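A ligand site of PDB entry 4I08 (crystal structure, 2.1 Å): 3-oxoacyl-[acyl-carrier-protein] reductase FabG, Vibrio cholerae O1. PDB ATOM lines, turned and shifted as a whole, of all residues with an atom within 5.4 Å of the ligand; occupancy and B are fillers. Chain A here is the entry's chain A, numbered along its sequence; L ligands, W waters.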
ATOM      1  N   THR A  18     -24.942 -24.973  -2.583  1.00  0.00           N
ATOM      2  CA  THR A  18     -26.065 -24.775  -1.660  1.00  0.00           C
ATOM      3  C   THR A  18     -25.785 -23.543  -0.835  1.00  0.00           C
ATOM      4  O   THR A  18     -24.618 -23.279  -0.500  1.00  0.00           O
ATOM      5  CB  THR A  18     -26.333 -26.009  -0.754  1.00  0.00           C
ATOM      6  OG1 THR A  18     -25.180 -26.300   0.053  1.00  0.00           O
ATOM      7  CG2 THR A  18     -26.635 -27.242  -1.638  1.00  0.00           C
ATOM      8  N   GLY A  19     -26.820 -22.782  -0.507  1.00  0.00           N
ATOM      9  CA  GLY A  19     -26.676 -21.594   0.334  1.00  0.00           C
ATOM     10  C   GLY A  19     -25.835 -20.535  -0.328  1.00  0.00           C
ATOM     11  O   GLY A  19     -24.847 -20.078   0.245  1.00  0.00           O
ATOM     12  N   ALA A  20     -26.235 -20.129  -1.542  1.00  0.00           N
ATOM     13  CA  ALA A  20     -25.413 -19.263  -2.363  1.00  0.00           C
ATOM     14  C   ALA A  20     -25.950 -17.818  -2.411  1.00  0.00           C
ATOM     15  O   ALA A  20     -25.524 -17.030  -3.253  1.00  0.00           O
ATOM     16  CB  ALA A  20     -25.314 -19.822  -3.778  1.00  0.00           C
ATOM     17  N   SER A  21     -26.876 -17.479  -1.517  1.00  0.00           N
ATOM     18  CA  SER A  21     -27.524 -16.156  -1.599  1.00  0.00           C
ATOM     19  C   SER A  21     -26.671 -15.039  -1.021  1.00  0.00           C
ATOM     20  O   SER A  21     -26.863 -13.861  -1.355  1.00  0.00           O
ATOM     21  CB  SER A  21     -28.935 -16.146  -1.002  1.00  0.00           C
ATOM     22  OG  SER A  21     -29.026 -16.761   0.265  1.00  0.00           O
ATOM     23  N   ARG A  22     -25.712 -15.389  -0.185  1.00  0.00           N
ATOM     24  CA  ARG A  22     -24.863 -14.403   0.444  1.00  0.00           C
ATOM     25  C   ARG A  22     -23.570 -15.040   0.945  1.00  0.00           C
ATOM     26  O   ARG A  22     -23.354 -16.265   0.827  1.00  0.00           O
ATOM     27  CB  ARG A  22     -25.606 -13.675   1.579  1.00  0.00           C
ATOM     28  CG  ARG A  22     -26.312 -14.601   2.575  1.00  0.00           C
ATOM     29  CD  ARG A  22     -27.564 -13.962   3.183  1.00  0.00           C
ATOM     30  NE  ARG A  22     -28.389 -14.959   3.875  1.00  0.00           N
ATOM     31  CZ  ARG A  22     -28.209 -15.356   5.139  1.00  0.00           C
ATOM     32  NH1 ARG A  22     -27.248 -14.842   5.893  1.00  0.00           N
ATOM     33  NH2 ARG A  22     -29.019 -16.281   5.669  1.00  0.00           N
ATOM     34  N   GLY A  23     -22.688 -14.171   1.412  1.00  0.00           N
ATOM     35  CA  GLY A  23     -21.424 -14.561   2.004  1.00  0.00           C
ATOM     36  C   GLY A  23     -20.577 -15.500   1.166  1.00  0.00           C
ATOM     37  O   GLY A  23     -20.257 -15.225  -0.011  1.00  0.00           O
ATOM     38  N   ILE A  24     -20.168 -16.587   1.799  1.00  0.00           N
ATOM     39  CA  ILE A  24     -19.197 -17.525   1.245  1.00  0.00           C
ATOM     40  C   ILE A  24     -19.789 -18.294   0.093  1.00  0.00           C
ATOM     41  O   ILE A  24     -19.118 -18.537  -0.889  1.00  0.00           O
ATOM     42  CB  ILE A  24     -18.677 -18.492   2.344  1.00  0.00           C
ATOM     43  CG1 ILE A  24     -17.710 -17.756   3.278  1.00  0.00           C
ATOM     44  CG2 ILE A  24     -18.001 -19.720   1.764  1.00  0.00           C
ATOM     45  CD1 ILE A  24     -17.553 -18.387   4.643  1.00  0.00           C
ATOM     46  N   GLY A  25     -21.054 -18.680   0.204  1.00  0.00           N
ATOM     47  CA  GLY A  25     -21.724 -19.416  -0.834  1.00  0.00           C
ATOM     48  C   GLY A  25     -21.885 -18.605  -2.110  1.00  0.00           C
ATOM     49  O   GLY A  25     -21.706 -19.107  -3.209  1.00  0.00           O
ATOM     50  N   THR A  42     -28.380 -22.051  -4.530  1.00  0.00           N
ATOM     51  CA  THR A  42     -29.664 -22.169  -3.849  1.00  0.00           C
ATOM     52  C   THR A  42     -29.763 -21.277  -2.614  1.00  0.00           C
ATOM     53  O   THR A  42     -28.766 -20.980  -1.951  1.00  0.00           O
ATOM     54  CB  THR A  42     -29.963 -23.616  -3.401  1.00  0.00           C
ATOM     55  OG1 THR A  42     -29.183 -23.924  -2.236  1.00  0.00           O
ATOM     56  CG2 THR A  42     -29.625 -24.615  -4.506  1.00  0.00           C
ATOM     57  N   ALA A  43     -31.003 -20.907  -2.327  1.00  0.00           N
ATOM     58  CA  ALA A  43     -31.436 -20.220  -1.116  1.00  0.00           C
ATOM     59  C   ALA A  43     -32.633 -20.972  -0.548  1.00  0.00           C
ATOM     60  O   ALA A  43     -33.122 -21.923  -1.174  1.00  0.00           O
ATOM     61  CB  ALA A  43     -31.834 -18.791  -1.441  1.00  0.00           C
ATOM     62  N   THR A  44     -33.110 -20.569   0.635  1.00  0.00           N
ATOM     63  CA  THR A  44     -34.231 -21.224   1.300  1.00  0.00           C
ATOM     64  C   THR A  44     -35.576 -20.632   0.901  1.00  0.00           C
ATOM     65  O   THR A  44     -36.611 -21.207   1.202  1.00  0.00           O
ATOM     66  CB  THR A  44     -34.131 -21.188   2.847  1.00  0.00           C
ATOM     67  OG1 THR A  44     -34.101 -19.840   3.313  1.00  0.00           O
ATOM     68  CG2 THR A  44     -32.863 -21.888   3.329  1.00  0.00           C
ATOM     69  N   SER A  45     -35.570 -19.494   0.208  1.00  0.00           N
ATOM     70  CA  SER A  45     -36.772 -18.857  -0.287  1.00  0.00           C
ATOM     71  C   SER A  45     -36.670 -18.572  -1.784  1.00  0.00           C
ATOM     72  O   SER A  45     -35.590 -18.585  -2.366  1.00  0.00           O
ATOM     73  CB  SER A  45     -37.046 -17.550   0.474  1.00  0.00           C
ATOM     74  OG  SER A  45     -36.096 -16.541   0.126  1.00  0.00           O
ATOM     75  N   LEU A  65     -34.082 -24.265  -2.085  1.00  0.00           N
ATOM     76  CA  LEU A  65     -33.715 -25.567  -1.508  1.00  0.00           C
ATOM     77  C   LEU A  65     -33.631 -25.492   0.009  1.00  0.00           C
ATOM     78  O   LEU A  65     -32.999 -24.588   0.568  1.00  0.00           O
ATOM     79  CB  LEU A  65     -32.396 -26.059  -2.080  1.00  0.00           C
ATOM     80  CG  LEU A  65     -31.857 -27.394  -1.552  1.00  0.00           C
ATOM     81  CD1 LEU A  65     -32.741 -28.545  -2.009  1.00  0.00           C
ATOM     82  CD2 LEU A  65     -30.439 -27.615  -2.009  1.00  0.00           C
ATOM     83  N   ASN A  66     -34.279 -26.452   0.672  1.00  0.00           N
ATOM     84  CA  ASN A  66     -34.065 -26.726   2.084  1.00  0.00           C
ATOM     85  C   ASN A  66     -33.308 -28.049   2.142  1.00  0.00           C
ATOM     86  O   ASN A  66     -33.866 -29.097   1.780  1.00  0.00           O
ATOM     87  CB  ASN A  66     -35.405 -26.850   2.839  1.00  0.00           C
ATOM     88  CG  ASN A  66     -35.239 -27.339   4.263  1.00  0.00           C
ATOM     89  OD1 ASN A  66     -34.137 -27.333   4.822  1.00  0.00           O
ATOM     90  ND2 ASN A  66     -36.325 -27.769   4.876  1.00  0.00           N
ATOM     91  N   VAL A  67     -32.054 -28.007   2.583  1.00  0.00           N
ATOM     92  CA  VAL A  67     -31.166 -29.185   2.534  1.00  0.00           C
ATOM     93  C   VAL A  67     -31.535 -30.259   3.564  1.00  0.00           C
ATOM     94  O   VAL A  67     -30.965 -31.359   3.530  1.00  0.00           O
ATOM     95  CB  VAL A  67     -29.664 -28.847   2.662  1.00  0.00           C
ATOM     96  CG1 VAL A  67     -29.224 -27.927   1.539  1.00  0.00           C
ATOM     97  CG2 VAL A  67     -29.318 -28.234   4.026  1.00  0.00           C
ATOM     98  N   THR A  68     -32.479 -29.942   4.459  1.00  0.00           N
ATOM     99  CA  THR A  68     -33.011 -30.912   5.437  1.00  0.00           C
ATOM    100  C   THR A  68     -34.253 -31.615   4.937  1.00  0.00           C
ATOM    101  O   THR A  68     -34.813 -32.446   5.635  1.00  0.00           O
ATOM    102  CB  THR A  68     -33.384 -30.258   6.795  1.00  0.00           C
ATOM    103  OG1 THR A  68     -34.574 -29.471   6.669  1.00  0.00           O
ATOM    104  CG2 THR A  68     -32.245 -29.404   7.330  1.00  0.00           C
ATOM    105  N   ASN A  93     -22.376 -25.996   1.052  1.00  0.00           N
ATOM    106  CA  ASN A  93     -22.036 -24.789   1.804  1.00  0.00           C
ATOM    107  C   ASN A  93     -23.069 -24.431   2.843  1.00  0.00           C
ATOM    108  O   ASN A  93     -22.732 -23.969   3.908  1.00  0.00           O
ATOM    109  CB  ASN A  93     -21.814 -23.619   0.850  1.00  0.00           C
ATOM    110  CG  ASN A  93     -21.720 -22.286   1.574  1.00  0.00           C
ATOM    111  OD1 ASN A  93     -20.696 -21.986   2.166  1.00  0.00           O
ATOM    112  ND2 ASN A  93     -22.778 -21.485   1.512  1.00  0.00           N
ATOM    113  N   ALA A  94     -24.324 -24.704   2.543  1.00  0.00           N
ATOM    114  CA  ALA A  94     -25.396 -24.400   3.473  1.00  0.00           C
ATOM    115  C   ALA A  94     -25.090 -24.876   4.902  1.00  0.00           C
ATOM    116  O   ALA A  94     -24.695 -26.014   5.146  1.00  0.00           O
ATOM    117  CB  ALA A  94     -26.698 -25.009   2.965  1.00  0.00           C
ATOM    118  N   GLY A  95     -25.283 -23.983   5.870  1.00  0.00           N
ATOM    119  CA  GLY A  95     -25.110 -24.362   7.254  1.00  0.00           C
ATOM    120  C   GLY A  95     -25.506 -23.258   8.201  1.00  0.00           C
ATOM    121  O   GLY A  95     -25.679 -22.108   7.797  1.00  0.00           O
ATOM    122  N   ILE A  96     -25.622 -23.614   9.469  1.00  0.00           N
ATOM    123  CA  ILE A  96     -26.100 -22.669  10.481  1.00  0.00           C
ATOM    124  C   ILE A  96     -25.306 -22.865  11.755  1.00  0.00           C
ATOM    125  O   ILE A  96     -24.615 -23.893  11.905  1.00  0.00           O
ATOM    126  CB  ILE A  96     -27.591 -22.896  10.822  1.00  0.00           C
ATOM    127  CG1 ILE A  96     -27.848 -24.380  11.217  1.00  0.00           C
ATOM    128  CG2 ILE A  96     -28.485 -22.549   9.642  1.00  0.00           C
ATOM    129  CD1 ILE A  96     -29.203 -24.635  11.832  1.00  0.00           C
ATOM    130  N   THR A 116     -28.851 -29.920   9.534  1.00  0.00           N
ATOM    131  CA  THR A 116     -28.485 -28.897   8.554  1.00  0.00           C
ATOM    132  C   THR A 116     -27.026 -29.004   8.135  1.00  0.00           C
ATOM    133  O   THR A 116     -26.711 -28.889   6.948  1.00  0.00           O
ATOM    134  CB  THR A 116     -28.743 -27.457   9.073  1.00  0.00           C
ATOM    135  OG1 THR A 116     -30.043 -27.375   9.635  1.00  0.00           O
ATOM    136  CG2 THR A 116     -28.657 -26.420   7.956  1.00  0.00           C
ATOM    137  N   ASN A 117     -26.145 -29.211   9.095  1.00  0.00           N
ATOM    138  CA  ASN A 117     -24.723 -29.181   8.808  1.00  0.00           C
ATOM    139  C   ASN A 117     -24.080 -30.544   8.510  1.00  0.00           C
ATOM    140  O   ASN A 117     -22.967 -30.554   7.997  1.00  0.00           O
ATOM    141  CB  ASN A 117     -23.946 -28.474   9.921  1.00  0.00           C
ATOM    142  CG  ASN A 117     -24.345 -26.997  10.077  1.00  0.00           C
ATOM    143  OD1 ASN A 117     -25.340 -26.550   9.542  1.00  0.00           O
ATOM    144  ND2 ASN A 117     -23.576 -26.250  10.890  1.00  0.00           N
ATOM    145  N   VAL A 143     -17.890 -27.308   2.776  1.00  0.00           N
ATOM    146  CA  VAL A 143     -17.434 -26.160   3.533  1.00  0.00           C
ATOM    147  C   VAL A 143     -17.570 -26.539   4.981  1.00  0.00           C
ATOM    148  O   VAL A 143     -18.678 -26.679   5.494  1.00  0.00           O
ATOM    149  CB  VAL A 143     -18.219 -24.890   3.187  1.00  0.00           C
ATOM    150  CG1 VAL A 143     -17.647 -23.690   3.948  1.00  0.00           C
ATOM    151  CG2 VAL A 143     -18.155 -24.628   1.681  1.00  0.00           C
ATOM    152  N   GLY A 144     -16.431 -26.760   5.629  1.00  0.00           N
ATOM    153  CA  GLY A 144     -16.374 -27.069   7.029  1.00  0.00           C
ATOM    154  C   GLY A 144     -16.125 -25.831   7.855  1.00  0.00           C
ATOM    155  O   GLY A 144     -16.658 -24.757   7.548  1.00  0.00           O
ATOM    156  N   SER A 145     -15.296 -25.993   8.888  1.00  0.00           N
ATOM    157  CA  SER A 145     -14.900 -24.892   9.768  1.00  0.00           C
ATOM    158  C   SER A 145     -13.678 -25.266  10.572  1.00  0.00           C
ATOM    159  O   SER A 145     -13.525 -26.417  10.988  1.00  0.00           O
ATOM    160  CB  SER A 145     -16.037 -24.534  10.722  1.00  0.00           C
ATOM    161  OG  SER A 145     -15.647 -23.543  11.662  1.00  0.00           O
ATOM    162  N   VAL A 146     -12.818 -24.278  10.820  1.00  0.00           N
ATOM    163  CA  VAL A 146     -11.690 -24.460  11.748  1.00  0.00           C
ATOM    164  C   VAL A 146     -12.149 -25.082  13.092  1.00  0.00           C
ATOM    165  O   VAL A 146     -11.382 -25.792  13.779  1.00  0.00           O
ATOM    166  CB  VAL A 146     -10.956 -23.123  11.981  1.00  0.00           C
ATOM    167  CG1 VAL A 146     -11.793 -22.182  12.829  1.00  0.00           C
ATOM    168  CG2 VAL A 146      -9.596 -23.352  12.608  1.00  0.00           C
ATOM    169  N   TYR A 158     -21.999 -27.516  16.695  1.00  0.00           N
ATOM    170  CA  TYR A 158     -21.385 -27.091  15.464  1.00  0.00           C
ATOM    171  C   TYR A 158     -20.075 -27.846  15.213  1.00  0.00           C
ATOM    172  O   TYR A 158     -19.822 -28.300  14.101  1.00  0.00           O
ATOM    173  CB  TYR A 158     -21.127 -25.589  15.548  1.00  0.00           C
ATOM    174  CG  TYR A 158     -20.629 -24.924  14.272  1.00  0.00           C
ATOM    175  CD1 TYR A 158     -21.510 -24.656  13.212  1.00  0.00           C
ATOM    176  CD2 TYR A 158     -19.329 -24.494  14.140  1.00  0.00           C
ATOM    177  CE1 TYR A 158     -21.083 -24.038  12.039  1.00  0.00           C
ATOM    178  CE2 TYR A 158     -18.891 -23.885  12.977  1.00  0.00           C
ATOM    179  CZ  TYR A 158     -19.779 -23.638  11.937  1.00  0.00           C
ATOM    180  OH  TYR A 158     -19.354 -22.991  10.784  1.00  0.00           O
ATOM    181  N   LYS A 162     -19.241 -30.348  12.126  1.00  0.00           N
ATOM    182  CA  LYS A 162     -18.171 -30.010  11.194  1.00  0.00           C
ATOM    183  C   LYS A 162     -17.053 -31.035  11.223  1.00  0.00           C
ATOM    184  O   LYS A 162     -16.467 -31.347  10.195  1.00  0.00           O
ATOM    185  CB  LYS A 162     -17.641 -28.622  11.476  1.00  0.00           C
ATOM    186  CG  LYS A 162     -18.676 -27.517  11.232  1.00  0.00           C
ATOM    187  CD  LYS A 162     -19.085 -27.443   9.770  1.00  0.00           C
ATOM    188  CE  LYS A 162     -19.782 -26.124   9.480  1.00  0.00           C
ATOM    189  NZ  LYS A 162     -20.150 -25.936   8.045  1.00  0.00           N
ATOM    190  N   PRO A 188     -12.881 -22.956   6.505  1.00  0.00           N
ATOM    191  CA  PRO A 188     -12.604 -21.533   6.810  1.00  0.00           C
ATOM    192  C   PRO A 188     -12.329 -21.259   8.298  1.00  0.00           C
ATOM    193  O   PRO A 188     -12.866 -21.927   9.165  1.00  0.00           O
ATOM    194  CB  PRO A 188     -13.899 -20.826   6.429  1.00  0.00           C
ATOM    195  CG  PRO A 188     -14.733 -21.800   5.699  1.00  0.00           C
ATOM    196  CD  PRO A 188     -14.278 -23.153   6.121  1.00  0.00           C
ATOM    197  N   GLY A 189     -11.522 -20.246   8.548  1.00  0.00           N
ATOM    198  CA  GLY A 189     -11.406 -19.665   9.863  1.00  0.00           C
ATOM    199  C   GLY A 189     -12.494 -18.637  10.052  1.00  0.00           C
ATOM    200  O   GLY A 189     -13.639 -18.849   9.656  1.00  0.00           O
ATOM    201  N   PHE A 190     -12.152 -17.520  10.674  1.00  0.00           N
ATOM    202  CA  PHE A 190     -13.144 -16.472  10.829  1.00  0.00           C
ATOM    203  C   PHE A 190     -13.130 -15.563   9.605  1.00  0.00           C
ATOM    204  O   PHE A 190     -12.122 -14.931   9.266  1.00  0.00           O
ATOM    205  CB  PHE A 190     -12.999 -15.758  12.172  1.00  0.00           C
ATOM    206  CG  PHE A 190     -13.655 -16.529  13.296  1.00  0.00           C
ATOM    207  CD1 PHE A 190     -14.857 -16.106  13.862  1.00  0.00           C
ATOM    208  CD2 PHE A 190     -13.114 -17.732  13.733  1.00  0.00           C
ATOM    209  CE1 PHE A 190     -15.462 -16.831  14.883  1.00  0.00           C
ATOM    210  CE2 PHE A 190     -13.718 -18.468  14.744  1.00  0.00           C
ATOM    211  CZ  PHE A 190     -14.892 -18.012  15.319  1.00  0.00           C
ATOM    212  N   ILE A 191     -14.270 -15.553   8.928  1.00  0.00           N
ATOM    213  CA  ILE A 191     -14.439 -14.863   7.633  1.00  0.00           C
ATOM    214  C   ILE A 191     -15.428 -13.715   7.827  1.00  0.00           C
ATOM    215  O   ILE A 191     -16.417 -13.854   8.535  1.00  0.00           O
ATOM    216  CB  ILE A 191     -14.999 -15.820   6.560  1.00  0.00           C
ATOM    217  CG1 ILE A 191     -14.235 -17.151   6.547  1.00  0.00           C
ATOM    218  CG2 ILE A 191     -15.026 -15.186   5.178  1.00  0.00           C
ATOM    219  CD1 ILE A 191     -12.748 -17.055   6.276  1.00  0.00           C
ATOM    220  N   THR A 193     -18.471 -12.184   7.296  1.00  0.00           N
ATOM    221  CA  THR A 193     -19.785 -12.643   6.829  1.00  0.00           C
ATOM    222  C   THR A 193     -20.822 -12.074   7.797  1.00  0.00           C
ATOM    223  O   THR A 193     -20.475 -11.360   8.741  1.00  0.00           O
ATOM    224  CB  THR A 193     -19.922 -14.194   6.878  1.00  0.00           C
ATOM    225  OG1 THR A 193     -19.445 -14.653   8.138  1.00  0.00           O
ATOM    226  CG2 THR A 193     -19.121 -14.887   5.781  1.00  0.00           C
ATOM    227  N   ASP A 194     -22.092 -12.360   7.577  1.00  0.00           N
ATOM    228  CA  ASP A 194     -23.111 -11.889   8.485  1.00  0.00           C
ATOM    229  C   ASP A 194     -22.637 -12.118   9.955  1.00  0.00           C
ATOM    230  O   ASP A 194     -22.313 -11.163  10.699  1.00  0.00           O
ATOM    231  CB  ASP A 194     -24.422 -12.610   8.188  1.00  0.00           C
ATOM    232  N   MET A 195     -22.534 -13.375  10.363  1.00  0.00           N
ATOM    233  CA  MET A 195     -21.980 -13.655  11.699  1.00  0.00           C
ATOM    234  C   MET A 195     -20.513 -13.180  11.810  1.00  0.00           C
ATOM    235  O   MET A 195     -20.215 -12.198  12.494  1.00  0.00           O
ATOM    236  CB  MET A 195     -22.060 -15.151  12.007  1.00  0.00           C
HETATM  237  P1  LIG L   1     -24.511 -17.246   6.030  1.00  0.00           P
HETATM  238  O1  LIG L   1     -23.874 -15.896   5.707  1.00  0.00           O
HETATM  239  O2  LIG L   1     -25.490 -17.385   7.157  1.00  0.00           O
HETATM  240  O3  LIG L   1     -25.338 -17.826   4.778  1.00  0.00           O
HETATM  241  C1  LIG L   1     -25.874 -19.146   4.947  1.00  0.00           C
HETATM  242  C2  LIG L   1     -26.356 -19.692   3.609  1.00  0.00           C
HETATM  243  O4  LIG L   1     -26.850 -21.007   3.815  1.00  0.00           O
HETATM  244  C3  LIG L   1     -27.510 -18.849   3.091  1.00  0.00           C
HETATM  245  O5  LIG L   1     -27.570 -18.822   1.662  1.00  0.00           O
HETATM  246  C4  LIG L   1     -28.732 -19.584   3.580  1.00  0.00           C
HETATM  247  O6  LIG L   1     -29.840 -19.249   2.751  1.00  0.00           O
HETATM  248  C5  LIG L   1     -28.251 -21.024   3.511  1.00  0.00           C
HETATM  249  N1  LIG L   1     -29.006 -21.914   4.419  1.00  0.00           N
HETATM  250  C6  LIG L   1     -29.163 -21.822   5.758  1.00  0.00           C
HETATM  251  N2  LIG L   1     -29.968 -22.847   6.168  1.00  0.00           N
HETATM  252  C7  LIG L   1     -30.291 -23.569   5.064  1.00  0.00           C
HETATM  253  C8  LIG L   1     -31.064 -24.710   4.862  1.00  0.00           C
HETATM  254  N3  LIG L   1     -31.689 -25.327   5.894  1.00  0.00           N
HETATM  255  N4  LIG L   1     -31.216 -25.194   3.609  1.00  0.00           N
HETATM  256  C9  LIG L   1     -30.599 -24.608   2.567  1.00  0.00           C
HETATM  257  N5  LIG L   1     -29.867 -23.491   2.721  1.00  0.00           N
HETATM  258  C10 LIG L   1     -29.697 -22.976   3.973  1.00  0.00           C
HETATM  259  O7  LIG L   1     -23.329 -18.356   6.167  1.00  0.00           O
HETATM  260  P2  LIG L   1     -21.750 -18.200   5.832  1.00  0.00           P
HETATM  261  O8  LIG L   1     -21.580 -17.757   4.391  1.00  0.00           O
HETATM  262  O9  LIG L   1     -21.013 -17.417   6.876  1.00  0.00           O
HETATM  263  O10 LIG L   1     -21.299 -19.733   6.004  1.00  0.00           O
HETATM  264  C11 LIG L   1     -21.545 -20.690   4.986  1.00  0.00           C
HETATM  265  C12 LIG L   1     -20.884 -21.972   5.458  1.00  0.00           C
HETATM  266  O11 LIG L   1     -19.563 -21.683   5.916  1.00  0.00           O
HETATM  267  C13 LIG L   1     -21.622 -22.600   6.626  1.00  0.00           C
HETATM  268  O12 LIG L   1     -21.580 -24.023   6.466  1.00  0.00           O
HETATM  269  C14 LIG L   1     -20.829 -22.194   7.849  1.00  0.00           C
HETATM  270  O13 LIG L   1     -21.002 -23.088   8.930  1.00  0.00           O
HETATM  271  C15 LIG L   1     -19.429 -22.185   7.262  1.00  0.00           C
HETATM  272  N6  LIG L   1     -18.507 -21.424   8.138  1.00  0.00           N
HETATM  273  C16 LIG L   1     -18.440 -20.040   7.972  1.00  0.00           C
HETATM  274  C17 LIG L   1     -17.580 -19.395   8.791  1.00  0.00           C
HETATM  275  C18 LIG L   1     -17.629 -17.963   9.031  1.00  0.00           C
HETATM  276  O14 LIG L   1     -16.582 -17.390   9.601  1.00  0.00           O
HETATM  277  N7  LIG L   1     -18.711 -17.255   8.670  1.00  0.00           N
HETATM  278  C19 LIG L   1     -16.568 -20.192   9.596  1.00  0.00           C
HETATM  279  C20 LIG L   1     -16.287 -21.459   8.845  1.00  0.00           C
HETATM  280  C21 LIG L   1     -17.254 -22.004   8.121  1.00  0.00           C
HETATM  281  P3  LIG L   1     -30.833 -18.001   3.075  1.00  0.00           P
HETATM  282  O15 LIG L   1     -32.098 -18.374   2.345  1.00  0.00           O
HETATM  283  O16 LIG L   1     -30.995 -17.980   4.585  1.00  0.00           O
HETATM  284  O17 LIG L   1     -30.069 -16.819   2.556  1.00  0.00           O
HETATM  285  O   HOH W   1     -21.866 -26.709   4.814  1.00  0.00           O
HETATM  286  O   HOH W   2     -30.656 -22.999   0.034  1.00  0.00           O
HETATM  287  O   HOH W   3     -33.748 -16.493   0.947  1.00  0.00           O
HETATM  288  O   HOH W   4     -27.084 -16.039   8.791  1.00  0.00           O
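NZ of Lys 162 sits at hydrogen-bond distance from O12 of the ligand (2.9 Å). OD1 of Asn 66 is in hydrogen-bond range of N3 of the ligand (3.3 Å). N of Ile 191 sits at hydrogen-bond distance from O14 of the ligand, at 3.0 Å. A nitrogen (N7) of the ligand is in hydrogen-bond range of the side-chain hydroxyl (OG1) of Thr 193 (2.8 Å). O of Asn 93 lies within hydrogen-bond range of O12 of the ligand. An oxygen (O13) of the ligand lies within hydrogen-bond range of the side-chain hydroxyl of Tyr 158 (2.5 Å). OG of Ser 21 sits at hydrogen-bond distance from O17 of the ligand (2.5 Å). The backbone carbonyl oxygen (O) of Gly 19 lies close to an oxygen (O5) of the ligand (3.3 Å). An oxygen (O16) of the ligand lies within salt-bridge range of the guanidinium group (NH2) of Arg 22 (2.8 Å). An oxygen (O8) of the ligand lies within hydrogen-bond range of the backbone NH of Ile 24 (3.2 Å). N of Val 67 is in hydrogen-bond range of N4 of the ligand (3.1 Å). The side-chain hydroxyl (OG1) of Thr 44 sits at hydrogen-bond distance from an oxygen (O15) of the ligand (2.7 Å). An oxygen (O15) of the ligand is in hydrogen-bond range of the backbone NH (N) of Thr 44 (3.0 Å).
Water W4 lies within hydrogen-bond range of an oxygen (O2) of the ligand and the guanidinium group of Arg 22. Water W3 bridges the side-chain hydroxyl of Ser 45 and an oxygen (O15) of the ligand.
The side-chain amide nitrogen (ND2) of Asn 93 lies within hydrogen-bond range of the backbone carbonyl oxygen (O) of Gly 19 (2.8 Å). The backbone NH of Val 146 is in hydrogen-bond range of the backbone carbonyl oxygen of Pro 188 (2.9 Å). N of Ala 20 sits at hydrogen-bond distance from O of Thr 42, 2.7 Å away. N of Gly 19 is in hydrogen-bond range of O of Thr 42, at 3.0 Å. OG1 of Thr 18 is in hydrogen-bond range of N of Asn 93 (3.0 Å). O of Ile 96 is in hydrogen-bond range of ND2 of Asn 117. OD1 of Asn 66 sits at hydrogen-bond distance from OG1 of Thr 68 (2.9 Å). The backbone carbonyl oxygen (O) of Val 143 sits at hydrogen-bond distance from the side-chain amino group (NZ) of Lys 162 (3.0 Å).
An oxygen (O14) of the ligand lies close to the backbone carbonyl oxygen (O) of Gly 189 (3.3 Å). Ala 20 touches the ligand (N to O5, 3.7 Å). Gly 23 touches the ligand (CA to O8, 3.99 Å). Ala 43 touches the ligand. Leu 65 touches the ligand. Ala 94 touches the ligand. Gly 95 touches the ligand (CA to O12, 3.6 Å). Ile 96 touches the ligand (CG2 to N2, 3.8 Å). Thr 116 touches the ligand. CG1 of Val 143 touches O11 of the ligand, at 3.4 Å. Gly 144 touches the ligand. Ser 145 touches the ligand (OG to C20, 3.6 Å). Pro 188 touches the ligand. Phe 190 touches the ligand (CA to O14, 3.8 Å).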
